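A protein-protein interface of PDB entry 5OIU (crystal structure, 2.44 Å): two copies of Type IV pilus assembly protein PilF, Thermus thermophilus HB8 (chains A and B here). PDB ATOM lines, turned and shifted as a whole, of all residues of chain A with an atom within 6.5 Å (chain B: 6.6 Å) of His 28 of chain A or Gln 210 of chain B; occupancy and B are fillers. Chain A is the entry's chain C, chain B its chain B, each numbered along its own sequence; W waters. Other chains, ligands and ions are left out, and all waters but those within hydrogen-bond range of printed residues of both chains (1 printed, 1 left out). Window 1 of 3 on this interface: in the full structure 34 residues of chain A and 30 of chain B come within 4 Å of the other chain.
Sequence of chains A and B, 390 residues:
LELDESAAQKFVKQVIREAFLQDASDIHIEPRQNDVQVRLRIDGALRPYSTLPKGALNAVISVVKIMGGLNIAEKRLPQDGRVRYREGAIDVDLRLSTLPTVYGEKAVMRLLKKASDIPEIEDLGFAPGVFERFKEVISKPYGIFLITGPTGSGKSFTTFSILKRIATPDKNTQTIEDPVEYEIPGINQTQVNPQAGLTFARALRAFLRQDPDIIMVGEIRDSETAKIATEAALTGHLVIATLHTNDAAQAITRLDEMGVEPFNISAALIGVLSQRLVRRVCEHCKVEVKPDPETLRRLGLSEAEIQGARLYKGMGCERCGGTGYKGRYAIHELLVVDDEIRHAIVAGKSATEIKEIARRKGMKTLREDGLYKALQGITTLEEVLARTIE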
ATOM      1  N   ASP A  26       4.053 -19.804  -0.333  1.00  0.00           N
ATOM      2  CA  ASP A  26       2.693 -20.188   0.048  1.00  0.00           C
ATOM      3  C   ASP A  26       1.839 -20.402  -1.200  1.00  0.00           C
ATOM      4  O   ASP A  26       2.072 -19.787  -2.247  1.00  0.00           O
ATOM      5  CB  ASP A  26       2.038 -19.122   0.947  1.00  0.00           C
ATOM      6  CG  ASP A  26       2.922 -18.721   2.141  1.00  0.00           C
ATOM      7  OD1 ASP A  26       2.870 -19.430   3.165  1.00  0.00           O
ATOM      8  OD2 ASP A  26       3.680 -17.717   2.067  1.00  0.00           O
ATOM      9  N   ILE A  27       0.827 -21.257  -1.064  1.00  0.00           N
ATOM     10  CA  ILE A  27      -0.148 -21.545  -2.117  1.00  0.00           C
ATOM     11  C   ILE A  27      -1.533 -21.222  -1.583  1.00  0.00           C
ATOM     12  O   ILE A  27      -1.959 -21.803  -0.572  1.00  0.00           O
ATOM     13  CB  ILE A  27      -0.102 -23.016  -2.550  1.00  0.00           C
ATOM     14  CG1 ILE A  27       1.302 -23.452  -2.929  1.00  0.00           C
ATOM     15  CG2 ILE A  27      -1.058 -23.264  -3.673  1.00  0.00           C
ATOM     16  CD1 ILE A  27       1.345 -24.916  -3.308  1.00  0.00           C
ATOM     17  N   HIS A  28      -2.251 -20.329  -2.273  1.00  0.00           N
ATOM     18  CA  HIS A  28      -3.608 -19.923  -1.895  1.00  0.00           C
ATOM     19  C   HIS A  28      -4.612 -20.424  -2.922  1.00  0.00           C
ATOM     20  O   HIS A  28      -4.499 -20.095  -4.111  1.00  0.00           O
ATOM     21  CB  HIS A  28      -3.742 -18.404  -1.801  1.00  0.00           C
ATOM     22  CG  HIS A  28      -2.865 -17.782  -0.767  1.00  0.00           C
ATOM     23  ND1 HIS A  28      -3.361 -17.003   0.254  1.00  0.00           N
ATOM     24  CD2 HIS A  28      -1.519 -17.804  -0.610  1.00  0.00           C
ATOM     25  CE1 HIS A  28      -2.360 -16.576   1.002  1.00  0.00           C
ATOM     26  NE2 HIS A  28      -1.231 -17.043   0.497  1.00  0.00           N
ATOM     27  N   ILE A  29      -5.623 -21.163  -2.455  1.00  0.00           N
ATOM     28  CA  ILE A  29      -6.707 -21.671  -3.291  1.00  0.00           C
ATOM     29  C   ILE A  29      -7.991 -20.995  -2.819  1.00  0.00           C
ATOM     30  O   ILE A  29      -8.626 -21.444  -1.852  1.00  0.00           O
ATOM     31  CB  ILE A  29      -6.800 -23.199  -3.237  1.00  0.00           C
ATOM     32  CG1 ILE A  29      -5.463 -23.788  -3.702  1.00  0.00           C
ATOM     33  CG2 ILE A  29      -7.931 -23.707  -4.124  1.00  0.00           C
ATOM     34  CD1 ILE A  29      -5.462 -25.286  -3.950  1.00  0.00           C
ATOM     35  N   GLU A  30      -8.378 -19.906  -3.495  1.00  0.00           N
ATOM     36  CA  GLU A  30      -9.473 -19.046  -3.061  1.00  0.00           C
ATOM     37  C   GLU A  30     -10.712 -19.242  -3.916  1.00  0.00           C
ATOM     38  O   GLU A  30     -10.707 -18.866  -5.096  1.00  0.00           O
ATOM     39  CB  GLU A  30      -9.068 -17.571  -3.111  1.00  0.00           C
ATOM     40  CG  GLU A  30      -7.636 -17.244  -2.704  1.00  0.00           C
ATOM     41  CD  GLU A  30      -7.458 -15.752  -2.427  1.00  0.00           C
ATOM     42  OE1 GLU A  30      -6.668 -15.393  -1.526  1.00  0.00           O
ATOM     43  OE2 GLU A  30      -8.126 -14.931  -3.111  1.00  0.00           O
ATOM     44  N   GLN A  37      -9.637 -18.952  -7.798  1.00  0.00           N
ATOM     45  CA  GLN A  37      -8.330 -18.465  -8.192  1.00  0.00           C
ATOM     46  C   GLN A  37      -7.267 -19.137  -7.336  1.00  0.00           C
ATOM     47  O   GLN A  37      -7.456 -19.338  -6.131  1.00  0.00           O
ATOM     48  CB  GLN A  37      -8.238 -16.940  -8.062  1.00  0.00           C
ATOM     49  CG  GLN A  37      -6.798 -16.401  -8.007  1.00  0.00           C
ATOM     50  CD  GLN A  37      -6.280 -15.883  -9.352  1.00  0.00           C
ATOM     51  OE1 GLN A  37      -6.670 -14.802  -9.802  1.00  0.00           O
ATOM     52  NE2 GLN A  37      -5.394 -16.657  -9.994  1.00  0.00           N
ATOM     53  N   VAL A  38      -6.168 -19.517  -7.979  1.00  0.00           N
ATOM     54  CA  VAL A  38      -4.995 -20.066  -7.314  1.00  0.00           C
ATOM     55  C   VAL A  38      -3.900 -19.018  -7.392  1.00  0.00           C
ATOM     56  O   VAL A  38      -3.597 -18.510  -8.477  1.00  0.00           O
ATOM     57  CB  VAL A  38      -4.557 -21.390  -7.964  1.00  0.00           C
ATOM     58  CG1 VAL A  38      -3.265 -21.930  -7.349  1.00  0.00           C
ATOM     59  CG2 VAL A  38      -5.666 -22.399  -7.845  1.00  0.00           C
ATOM     60  N   ARG A  39      -3.330 -18.669  -6.246  1.00  0.00           N
ATOM     61  CA  ARG A  39      -2.240 -17.708  -6.189  1.00  0.00           C
ATOM     62  C   ARG A  39      -1.042 -18.346  -5.503  1.00  0.00           C
ATOM     63  O   ARG A  39      -1.195 -19.223  -4.641  1.00  0.00           O
ATOM     64  CB  ARG A  39      -2.657 -16.429  -5.445  1.00  0.00           C
ATOM     65  CG  ARG A  39      -3.863 -15.678  -6.045  1.00  0.00           C
ATOM     66  CD  ARG A  39      -4.720 -14.986  -4.945  1.00  0.00           C
ATOM     67  NE  ARG A  39      -4.256 -13.631  -4.629  1.00  0.00           N
ATOM     68  CZ  ARG A  39      -4.715 -12.892  -3.618  1.00  0.00           C
ATOM     69  NH1 ARG A  39      -5.662 -13.362  -2.816  1.00  0.00           N
ATOM     70  NH2 ARG A  39      -4.227 -11.669  -3.408  1.00  0.00           N
ATOM     71  N   LEU A  40       0.156 -17.901  -5.894  1.00  0.00           N
ATOM     72  CA  LEU A  40       1.413 -18.299  -5.268  1.00  0.00           C
ATOM     73  C   LEU A  40       2.065 -17.055  -4.688  1.00  0.00           C
ATOM     74  O   LEU A  40       2.130 -16.029  -5.371  1.00  0.00           O
ATOM     75  CB  LEU A  40       2.370 -18.951  -6.286  1.00  0.00           C
ATOM     76  CG  LEU A  40       1.941 -20.198  -7.083  1.00  0.00           C
ATOM     77  CD1 LEU A  40       3.063 -20.742  -7.989  1.00  0.00           C
ATOM     78  CD2 LEU A  40       1.448 -21.310  -6.157  1.00  0.00           C
ATOM     79  N   ARG A  41       2.554 -17.128  -3.444  1.00  0.00           N
ATOM     80  CA  ARG A  41       3.446 -16.071  -2.952  1.00  0.00           C
ATOM     81  C   ARG A  41       4.893 -16.346  -3.395  1.00  0.00           C
ATOM     82  O   ARG A  41       5.520 -17.334  -2.972  1.00  0.00           O
ATOM     83  CB  ARG A  41       3.365 -15.909  -1.436  1.00  0.00           C
ATOM     84  CG  ARG A  41       3.842 -14.505  -1.008  1.00  0.00           C
ATOM     85  CD  ARG A  41       3.798 -14.234   0.498  1.00  0.00           C
ATOM     86  NE  ARG A  41       2.432 -14.214   1.027  1.00  0.00           N
ATOM     87  CZ  ARG A  41       1.670 -13.126   1.068  1.00  0.00           C
ATOM     88  NH1 ARG A  41       2.153 -11.972   0.608  1.00  0.00           N
ATOM     89  NH2 ARG A  41       0.437 -13.190   1.576  1.00  0.00           N
ATOM     90  N   LEU A  46       1.948 -11.990  -3.773  1.00  0.00           N
ATOM     91  CA  LEU A  46       1.046 -12.981  -4.338  1.00  0.00           C
ATOM     92  C   LEU A  46       0.856 -12.703  -5.824  1.00  0.00           C
ATOM     93  O   LEU A  46       0.583 -11.566  -6.232  1.00  0.00           O
ATOM     94  CB  LEU A  46      -0.299 -12.969  -3.606  1.00  0.00           C
ATOM     95  CG  LEU A  46      -0.291 -13.711  -2.266  1.00  0.00           C
ATOM     96  CD1 LEU A  46      -1.547 -13.419  -1.469  1.00  0.00           C
ATOM     97  CD2 LEU A  46      -0.123 -15.218  -2.485  1.00  0.00           C
ATOM     98  N   ARG A  95       2.552 -26.758   5.541  1.00  0.00           N
ATOM     99  CA  ARG A  95       1.554 -26.369   6.538  1.00  0.00           C
ATOM    100  C   ARG A  95       0.231 -26.118   5.816  1.00  0.00           C
ATOM    101  O   ARG A  95       0.124 -25.190   5.012  1.00  0.00           O
ATOM    102  CB  ARG A  95       2.035 -25.120   7.276  1.00  0.00           C
ATOM    103  CG  ARG A  95       1.372 -24.811   8.615  1.00  0.00           C
ATOM    104  CD  ARG A  95       0.140 -23.902   8.477  1.00  0.00           C
ATOM    105  NE  ARG A  95       0.350 -22.678   7.682  1.00  0.00           N
ATOM    106  CZ  ARG A  95       1.060 -21.623   8.085  1.00  0.00           C
ATOM    107  NH1 ARG A  95       1.650 -21.641   9.270  1.00  0.00           N
ATOM    108  NH2 ARG A  95       1.190 -20.558   7.295  1.00  0.00           N
ATOM    109  N   SER A  97      -3.899 -25.241   5.807  1.00  0.00           N
ATOM    110  CA  SER A  97      -4.938 -24.562   6.570  1.00  0.00           C
ATOM    111  C   SER A  97      -6.164 -24.388   5.693  1.00  0.00           C
ATOM    112  O   SER A  97      -6.048 -23.869   4.582  1.00  0.00           O
ATOM    113  CB  SER A  97      -4.451 -23.202   7.069  1.00  0.00           C
ATOM    114  OG  SER A  97      -5.522 -22.286   7.201  1.00  0.00           O
ATOM    115  N   THR A  98      -7.329 -24.836   6.170  1.00  0.00           N
ATOM    116  CA  THR A  98      -8.579 -24.639   5.449  1.00  0.00           C
ATOM    117  C   THR A  98      -9.498 -23.748   6.264  1.00  0.00           C
ATOM    118  O   THR A  98      -9.652 -23.936   7.475  1.00  0.00           O
ATOM    119  CB  THR A  98      -9.305 -25.956   5.124  1.00  0.00           C
ATOM    120  OG1 THR A  98      -9.758 -26.579   6.330  1.00  0.00           O
ATOM    121  CG2 THR A  98      -8.401 -26.900   4.346  1.00  0.00           C
ATOM    122  N   LEU A  99     -10.120 -22.784   5.588  1.00  0.00           N
ATOM    123  CA  LEU A  99     -10.902 -21.786   6.246  1.00  0.00           C
ATOM    124  C   LEU A  99     -12.200 -21.595   5.474  1.00  0.00           C
ATOM    125  O   LEU A  99     -12.162 -21.358   4.253  1.00  0.00           O
ATOM    126  CB  LEU A  99     -10.123 -20.478   6.324  1.00  0.00           C
ATOM    127  CG  LEU A  99     -10.844 -19.253   6.883  1.00  0.00           C
ATOM    128  CD1 LEU A  99     -10.661 -19.179   8.391  1.00  0.00           C
ATOM    129  CD2 LEU A  99     -10.319 -17.988   6.212  1.00  0.00           C
ATOM    130  N   THR A 101     -15.168 -19.637   3.872  1.00  0.00           N
ATOM    131  CA  THR A 101     -15.430 -18.293   3.389  1.00  0.00           C
ATOM    132  C   THR A 101     -16.831 -18.243   2.812  1.00  0.00           C
ATOM    133  O   THR A 101     -17.572 -19.233   2.803  1.00  0.00           O
ATOM    134  CB  THR A 101     -14.431 -17.829   2.318  1.00  0.00           C
ATOM    135  OG1 THR A 101     -14.712 -18.503   1.083  1.00  0.00           O
ATOM    136  CG2 THR A 101     -13.006 -18.108   2.750  1.00  0.00           C
ATOM    137  N   LYS A 106     -11.383 -21.958   1.603  1.00  0.00           N
ATOM    138  CA  LYS A 106     -10.105 -21.505   1.093  1.00  0.00           C
ATOM    139  C   LYS A 106      -9.021 -22.343   1.738  1.00  0.00           C
ATOM    140  O   LYS A 106      -9.076 -22.633   2.934  1.00  0.00           O
ATOM    141  CB  LYS A 106      -9.872 -20.022   1.383  1.00  0.00           C
ATOM    142  CG  LYS A 106      -8.447 -19.605   1.097  1.00  0.00           C
ATOM    143  CD  LYS A 106      -8.190 -18.120   1.239  1.00  0.00           C
ATOM    144  CE  LYS A 106      -6.737 -17.835   0.861  1.00  0.00           C
ATOM    145  NZ  LYS A 106      -6.364 -16.417   0.876  1.00  0.00           N
ATOM    146  N   ALA A 107      -8.053 -22.766   0.947  1.00  0.00           N
ATOM    147  CA  ALA A 107      -6.959 -23.562   1.472  1.00  0.00           C
ATOM    148  C   ALA A 107      -5.669 -22.785   1.282  1.00  0.00           C
ATOM    149  O   ALA A 107      -5.423 -22.241   0.200  1.00  0.00           O
ATOM    150  CB  ALA A 107      -6.899 -24.920   0.782  1.00  0.00           C
ATOM    151  N   VAL A 108      -4.864 -22.691   2.337  1.00  0.00           N
ATOM    152  CA  VAL A 108      -3.526 -22.121   2.236  1.00  0.00           C
ATOM    153  C   VAL A 108      -2.539 -23.223   2.576  1.00  0.00           C
ATOM    154  O   VAL A 108      -2.723 -23.953   3.560  1.00  0.00           O
ATOM    155  CB  VAL A 108      -3.329 -20.894   3.152  1.00  0.00           C
ATOM    156  CG1 VAL A 108      -1.866 -20.458   3.138  1.00  0.00           C
ATOM    157  CG2 VAL A 108      -4.205 -19.719   2.704  1.00  0.00           C
ATOM    158  N   MET A 109      -1.514 -23.369   1.746  1.00  0.00           N
ATOM    159  CA  MET A 109      -0.433 -24.300   2.027  1.00  0.00           C
ATOM    160  C   MET A 109       0.876 -23.522   2.062  1.00  0.00           C
ATOM    161  O   MET A 109       1.338 -23.031   1.025  1.00  0.00           O
ATOM    162  CB  MET A 109      -0.403 -25.416   0.987  1.00  0.00           C
ATOM    163  CG  MET A 109      -1.428 -26.506   1.249  1.00  0.00           C
ATOM    164  SD  MET A 109      -1.506 -27.781  -0.020  1.00  0.00           S
ATOM    165  CE  MET A 109      -1.760 -26.791  -1.498  1.00  0.00           C
ATOM    166  N   ARG A 110       1.463 -23.383   3.254  1.00  0.00           N
ATOM    167  CA  ARG A 110       2.774 -22.764   3.355  1.00  0.00           C
ATOM    168  C   ARG A 110       3.845 -23.816   3.135  1.00  0.00           C
ATOM    169  O   ARG A 110       3.821 -24.882   3.758  1.00  0.00           O
ATOM    170  CB  ARG A 110       3.001 -22.081   4.707  1.00  0.00           C
ATOM    171  CG  ARG A 110       4.503 -21.685   4.846  1.00  0.00           C
ATOM    172  CD  ARG A 110       4.814 -20.488   5.749  1.00  0.00           C
ATOM    173  NE  ARG A 110       4.165 -19.252   5.337  1.00  0.00           N
ATOM    174  CZ  ARG A 110       3.653 -18.392   6.211  1.00  0.00           C
ATOM    175  NH1 ARG A 110       3.746 -18.667   7.504  1.00  0.00           N
ATOM    176  NH2 ARG A 110       3.050 -17.276   5.816  1.00  0.00           N
ATOM    177  N   ASN B 172      -3.035 -10.802   0.373  1.00  0.00           N
ATOM    178  CA  ASN B 172      -4.179 -11.576   0.842  1.00  0.00           C
ATOM    179  C   ASN B 172      -4.904 -10.712   1.861  1.00  0.00           C
ATOM    180  O   ASN B 172      -4.339 -10.389   2.911  1.00  0.00           O
ATOM    181  CB  ASN B 172      -3.744 -12.898   1.467  1.00  0.00           C
ATOM    182  CG  ASN B 172      -4.928 -13.712   2.007  1.00  0.00           C
ATOM    183  OD1 ASN B 172      -6.077 -13.524   1.602  1.00  0.00           O
ATOM    184  ND2 ASN B 172      -4.641 -14.631   2.923  1.00  0.00           N
ATOM    185  N   GLN B 174      -8.258 -10.502   4.289  1.00  0.00           N
ATOM    186  CA  GLN B 174      -9.153 -11.479   4.903  1.00  0.00           C
ATOM    187  C   GLN B 174      -9.908 -10.801   6.028  1.00  0.00           C
ATOM    188  O   GLN B 174      -9.316 -10.042   6.800  1.00  0.00           O
ATOM    189  CB  GLN B 174      -8.370 -12.695   5.416  1.00  0.00           C
ATOM    190  CG  GLN B 174      -9.165 -13.732   6.194  1.00  0.00           C
ATOM    191  CD  GLN B 174     -10.038 -14.582   5.303  1.00  0.00           C
ATOM    192  OE1 GLN B 174      -9.550 -15.218   4.376  1.00  0.00           O
ATOM    193  NE2 GLN B 174     -11.339 -14.597   5.575  1.00  0.00           N
ATOM    194  N   ASN B 188     -11.193 -11.721   0.707  1.00  0.00           N
ATOM    195  CA  ASN B 188     -11.742 -12.963   1.238  1.00  0.00           C
ATOM    196  C   ASN B 188     -12.584 -12.664   2.473  1.00  0.00           C
ATOM    197  O   ASN B 188     -12.133 -11.958   3.379  1.00  0.00           O
ATOM    198  CB  ASN B 188     -10.627 -13.951   1.586  1.00  0.00           C
ATOM    199  CG  ASN B 188      -9.792 -14.360   0.377  1.00  0.00           C
ATOM    200  OD1 ASN B 188     -10.300 -14.925  -0.587  1.00  0.00           O
ATOM    201  ND2 ASN B 188      -8.505 -14.093   0.440  1.00  0.00           N
ATOM    202  N   ARG B 205      -7.700 -16.846  15.020  1.00  0.00           N
ATOM    203  CA  ARG B 205      -6.593 -17.785  15.152  1.00  0.00           C
ATOM    204  C   ARG B 205      -6.334 -18.492  13.841  1.00  0.00           C
ATOM    205  O   ARG B 205      -5.180 -18.678  13.445  1.00  0.00           O
ATOM    206  CB  ARG B 205      -6.872 -18.795  16.263  1.00  0.00           C
ATOM    207  CG  ARG B 205      -6.340 -18.312  17.567  1.00  0.00           C
ATOM    208  CD  ARG B 205      -6.356 -19.360  18.612  1.00  0.00           C
ATOM    209  NE  ARG B 205      -6.495 -18.750  19.930  1.00  0.00           N
ATOM    210  CZ  ARG B 205      -7.663 -18.567  20.542  1.00  0.00           C
ATOM    211  NH1 ARG B 205      -8.802 -18.951  19.955  1.00  0.00           N
ATOM    212  NH2 ARG B 205      -7.690 -17.995  21.743  1.00  0.00           N
ATOM    213  N   ALA B 206      -7.396 -18.874  13.140  1.00  0.00           N
ATOM    214  CA  ALA B 206      -7.218 -19.545  11.864  1.00  0.00           C
ATOM    215  C   ALA B 206      -6.548 -18.632  10.840  1.00  0.00           C
ATOM    216  O   ALA B 206      -5.741 -19.101  10.025  1.00  0.00           O
ATOM    217  CB  ALA B 206      -8.569 -20.038  11.353  1.00  0.00           C
ATOM    218  N   PHE B 207      -6.868 -17.323  10.867  1.00  0.00           N
ATOM    219  CA  PHE B 207      -6.299 -16.383   9.894  1.00  0.00           C
ATOM    220  C   PHE B 207      -4.775 -16.393   9.943  1.00  0.00           C
ATOM    221  O   PHE B 207      -4.105 -16.303   8.905  1.00  0.00           O
ATOM    222  CB  PHE B 207      -6.812 -14.962  10.150  1.00  0.00           C
ATOM    223  CG  PHE B 207      -8.269 -14.755   9.838  1.00  0.00           C
ATOM    224  CD1 PHE B 207      -9.064 -15.799   9.405  1.00  0.00           C
ATOM    225  CD2 PHE B 207      -8.830 -13.501   9.953  1.00  0.00           C
ATOM    226  CE1 PHE B 207     -10.380 -15.606   9.114  1.00  0.00           C
ATOM    227  CE2 PHE B 207     -10.152 -13.286   9.642  1.00  0.00           C
ATOM    228  CZ  PHE B 207     -10.940 -14.344   9.238  1.00  0.00           C
ATOM    229  N   LEU B 208      -4.208 -16.524  11.145  1.00  0.00           N
ATOM    230  CA  LEU B 208      -2.758 -16.554  11.326  1.00  0.00           C
ATOM    231  C   LEU B 208      -2.069 -17.729  10.638  1.00  0.00           C
ATOM    232  O   LEU B 208      -0.844 -17.685  10.447  1.00  0.00           O
ATOM    233  CB  LEU B 208      -2.428 -16.554  12.807  1.00  0.00           C
ATOM    234  CG  LEU B 208      -3.076 -15.364  13.506  1.00  0.00           C
ATOM    235  CD1 LEU B 208      -2.747 -15.418  14.973  1.00  0.00           C
ATOM    236  CD2 LEU B 208      -2.530 -14.105  12.899  1.00  0.00           C
ATOM    237  N   ARG B 209      -2.809 -18.770  10.249  1.00  0.00           N
ATOM    238  CA  ARG B 209      -2.285 -19.828   9.391  1.00  0.00           C
ATOM    239  C   ARG B 209      -2.697 -19.647   7.924  1.00  0.00           C
ATOM    240  O   ARG B 209      -2.457 -20.533   7.099  1.00  0.00           O
ATOM    241  CB  ARG B 209      -2.735 -21.193   9.930  1.00  0.00           C
ATOM    242  CG  ARG B 209      -2.959 -21.244  11.477  1.00  0.00           C
ATOM    243  CD  ARG B 209      -3.993 -22.357  11.864  1.00  0.00           C
ATOM    244  NE  ARG B 209      -4.813 -22.138  13.085  1.00  0.00           N
ATOM    245  CZ  ARG B 209      -6.034 -22.660  13.317  1.00  0.00           C
ATOM    246  NH1 ARG B 209      -6.663 -22.388  14.450  1.00  0.00           N
ATOM    247  NH2 ARG B 209      -6.643 -23.448  12.426  1.00  0.00           N
ATOM    248  N   GLN B 210      -3.317 -18.519   7.583  1.00  0.00           N
ATOM    249  CA  GLN B 210      -3.811 -18.279   6.238  1.00  0.00           C
ATOM    250  C   GLN B 210      -2.918 -17.330   5.463  1.00  0.00           C
ATOM    251  O   GLN B 210      -3.336 -16.811   4.426  1.00  0.00           O
ATOM    252  CB  GLN B 210      -5.235 -17.726   6.279  1.00  0.00           C
ATOM    253  CG  GLN B 210      -6.319 -18.766   6.507  1.00  0.00           C
ATOM    254  CD  GLN B 210      -6.779 -19.397   5.206  1.00  0.00           C
ATOM    255  OE1 GLN B 210      -7.129 -18.696   4.253  1.00  0.00           O
ATOM    256  NE2 GLN B 210      -6.778 -20.721   5.159  1.00  0.00           N
ATOM    257  N   ASP B 211      -1.703 -17.086   5.943  1.00  0.00           N
ATOM    258  CA  ASP B 211      -0.735 -16.251   5.250  1.00  0.00           C
ATOM    259  C   ASP B 211      -1.377 -14.910   4.855  1.00  0.00           C
ATOM    260  O   ASP B 211      -1.363 -14.525   3.693  1.00  0.00           O
ATOM    261  CB  ASP B 211      -0.193 -16.984   4.027  1.00  0.00           C
ATOM    262  CG  ASP B 211       0.819 -16.182   3.257  1.00  0.00           C
ATOM    263  OD1 ASP B 211       1.595 -15.447   3.908  1.00  0.00           O
ATOM    264  OD2 ASP B 211       0.791 -16.246   2.001  1.00  0.00           O
ATOM    265  N   PRO B 212      -1.968 -14.199   5.814  1.00  0.00           N
ATOM    266  CA  PRO B 212      -2.604 -12.926   5.484  1.00  0.00           C
ATOM    267  C   PRO B 212      -1.574 -11.830   5.247  1.00  0.00           C
ATOM    268  O   PRO B 212      -0.423 -11.901   5.679  1.00  0.00           O
ATOM    269  CB  PRO B 212      -3.414 -12.622   6.746  1.00  0.00           C
ATOM    270  CG  PRO B 212      -2.503 -13.121   7.831  1.00  0.00           C
ATOM    271  CD  PRO B 212      -1.832 -14.363   7.272  1.00  0.00           C
ATOM    272  N   ASP B 213      -2.022 -10.789   4.556  1.00  0.00           N
ATOM    273  CA  ASP B 213      -1.364  -9.491   4.639  1.00  0.00           C
ATOM    274  C   ASP B 213      -2.198  -8.466   5.384  1.00  0.00           C
ATOM    275  O   ASP B 213      -1.678  -7.745   6.228  1.00  0.00           O
ATOM    276  CB  ASP B 213      -1.038  -8.974   3.240  1.00  0.00           C
ATOM    277  CG  ASP B 213      -0.033  -9.866   2.519  1.00  0.00           C
ATOM    278  OD1 ASP B 213       1.177  -9.838   2.873  1.00  0.00           O
ATOM    279  OD2 ASP B 213      -0.473 -10.594   1.605  1.00  0.00           O
HETATM  280  O   HOH W   1      -7.079 -16.054   3.658  1.00  0.00           O
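Water W1 lies within hydrogen-bond range of OE1 of Gln 174 of chain B (2.7 Å), OE1 of Gln 210 of chain B (2.7 Å), NZ of Lys 106 of chain A (2.9 Å) and ND2 of Asn 172 of chain B (2.9 Å).
No position is printed for both chains.
Among the printed residues, pairs that only touch across the chains: Lys 106 of chain A with Gln 210 of chain B (3.2 Å), Ser 97 of chain A with Arg 209 of chain B (3.3 Å), Leu 99 of chain A with Gln 174 of chain B (3.4 Å), Val 108 of chain A with Gln 210 of chain B (3.5 Å), Leu 46 of chain A with Asn 172 of chain B (3.5 Å), Leu 99 of chain A with Gln 210 of chain B (3.6 Å), His 28 of chain A with Asn 172 of chain B (3.6 Å), His 28 of chain A with Gln 210 of chain B (3.6 Å), Arg 95 of chain A with Arg 209 of chain B (3.6 Å), Leu 99 of chain A with Phe 207 of chain B (3.7 Å), Glu 30 of chain A with Asn 172 of chain B (3.7 Å), Leu 99 of chain A with Ala 206 of chain B (3.7 Å) and Val 108 of chain A with Asp 211 of chain B (3.96 Å).
The side-chain amide oxygen (OD1) of Asn 172 of chain B is in hydrogen-bond range of the side-chain amide nitrogen (ND2) of Asn 188 of chain B (2.8 Å). The side-chain amide nitrogen (ND2) of Asn 172 of chain B is in hydrogen-bond range of the backbone carbonyl oxygen (O) of Gln 210 of chain B, 3.0 Å away. ND2 of Asn 172 of chain B lies within hydrogen-bond range of O of Asp 211 of chain B, 3.4 Å away. The backbone NH (N) of Glu 30 of chain A is in hydrogen-bond range of the backbone carbonyl oxygen (O) of Gln 37 of chain A. The side-chain carboxylate (OE1) of Glu 30 of chain A lies within salt-bridge range of the side-chain amino group (NZ) of Lys 106 of chain A. The backbone NH (N) of Val 108 of chain A sits at hydrogen-bond distance from the backbone carbonyl oxygen (O) of Ser 97 of chain A (2.8 Å).
Printed residues of chain A that touch a printed residue of chain B: Asp 26, His 28, Glu 30, Arg 41, Leu 46, Arg 95, Ser 97, Leu 99, Lys 106, Val 108 and Arg 110. Of the 12 printed residues of chain B, 9 touch a printed residue of chain A. Among the printed residues, 22 pairs touch across the chains.
NZ of Lys 106 of chain A sits at hydrogen-bond distance from OD1 of Asn 172 of chain B (3.0 Å). The side-chain amide nitrogen (ND2) of Asn 188 of chain B sits at hydrogen-bond distance from the side-chain carboxylate (OE1) of Glu 30 of chain A (3.0 Å). The side-chain amide nitrogen of Asn 188 of chain B lies close to the side-chain amino group of Lys 106 of chain A. The side-chain hydroxyl of Ser 97 of chain A lies within hydrogen-bond range of the side-chain amide nitrogen of Gln 210 of chain B (2.9 Å). A ring nitrogen (NE2) of His 28 of chain A is in hydrogen-bond range of the side-chain carboxylate (OD2) of Asp 211 of chain B (2.6 Å). The guanidinium group of Arg 41 of chain A is in salt-bridge range of the side-chain carboxylate of Asp 211 of chain B (2.8 Å). NH2 of Arg 110 of chain A is in salt-bridge range of OD1 of Asp 211 of chain B (3.0 Å). The side-chain carboxylate (OD2) of Asp 213 of chain B is in salt-bridge range of the guanidinium group (NH2) of Arg 41 of chain A (2.8 Å). The side-chain carboxylate of Asp 211 of chain B sits close to the side-chain carboxylate of Asp 26 of chain A (3.2 Å).
His 28 of chain A touches three residues of chain B. Of the printed residues of chain B, Leu 46 of chain A touches Asn 172 (3.5 Å). Of the printed residues of chain B, Arg 95 of chain A touches Arg 209 (3.6 Å). Of the printed residues of chain B, Ser 97 of chain A touches Arg 209 (3.3 Å) and Gln 210 (2.9 Å). Ala 107 of chain A touches none of the printed residues of chain B. Printed residues of chain B within 4 Å of Val 108 of chain A: Gln 210 (3.5 Å) and Asp 211 (3.96 Å). Pro 212 of chain B touches none of the printed residues of chain A. The nearest residue of chain B that does not touch His 28 of chain A is Pro 212 of chain B (5.4 Å). The nearest residue of chain A that does not touch Gln 210 of chain B is Thr 98 of chain A (4.2 Å). The nearest printed residue of chain A that does not touch Gln 174 of chain B is Lys 106 of chain A (4.5 Å).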
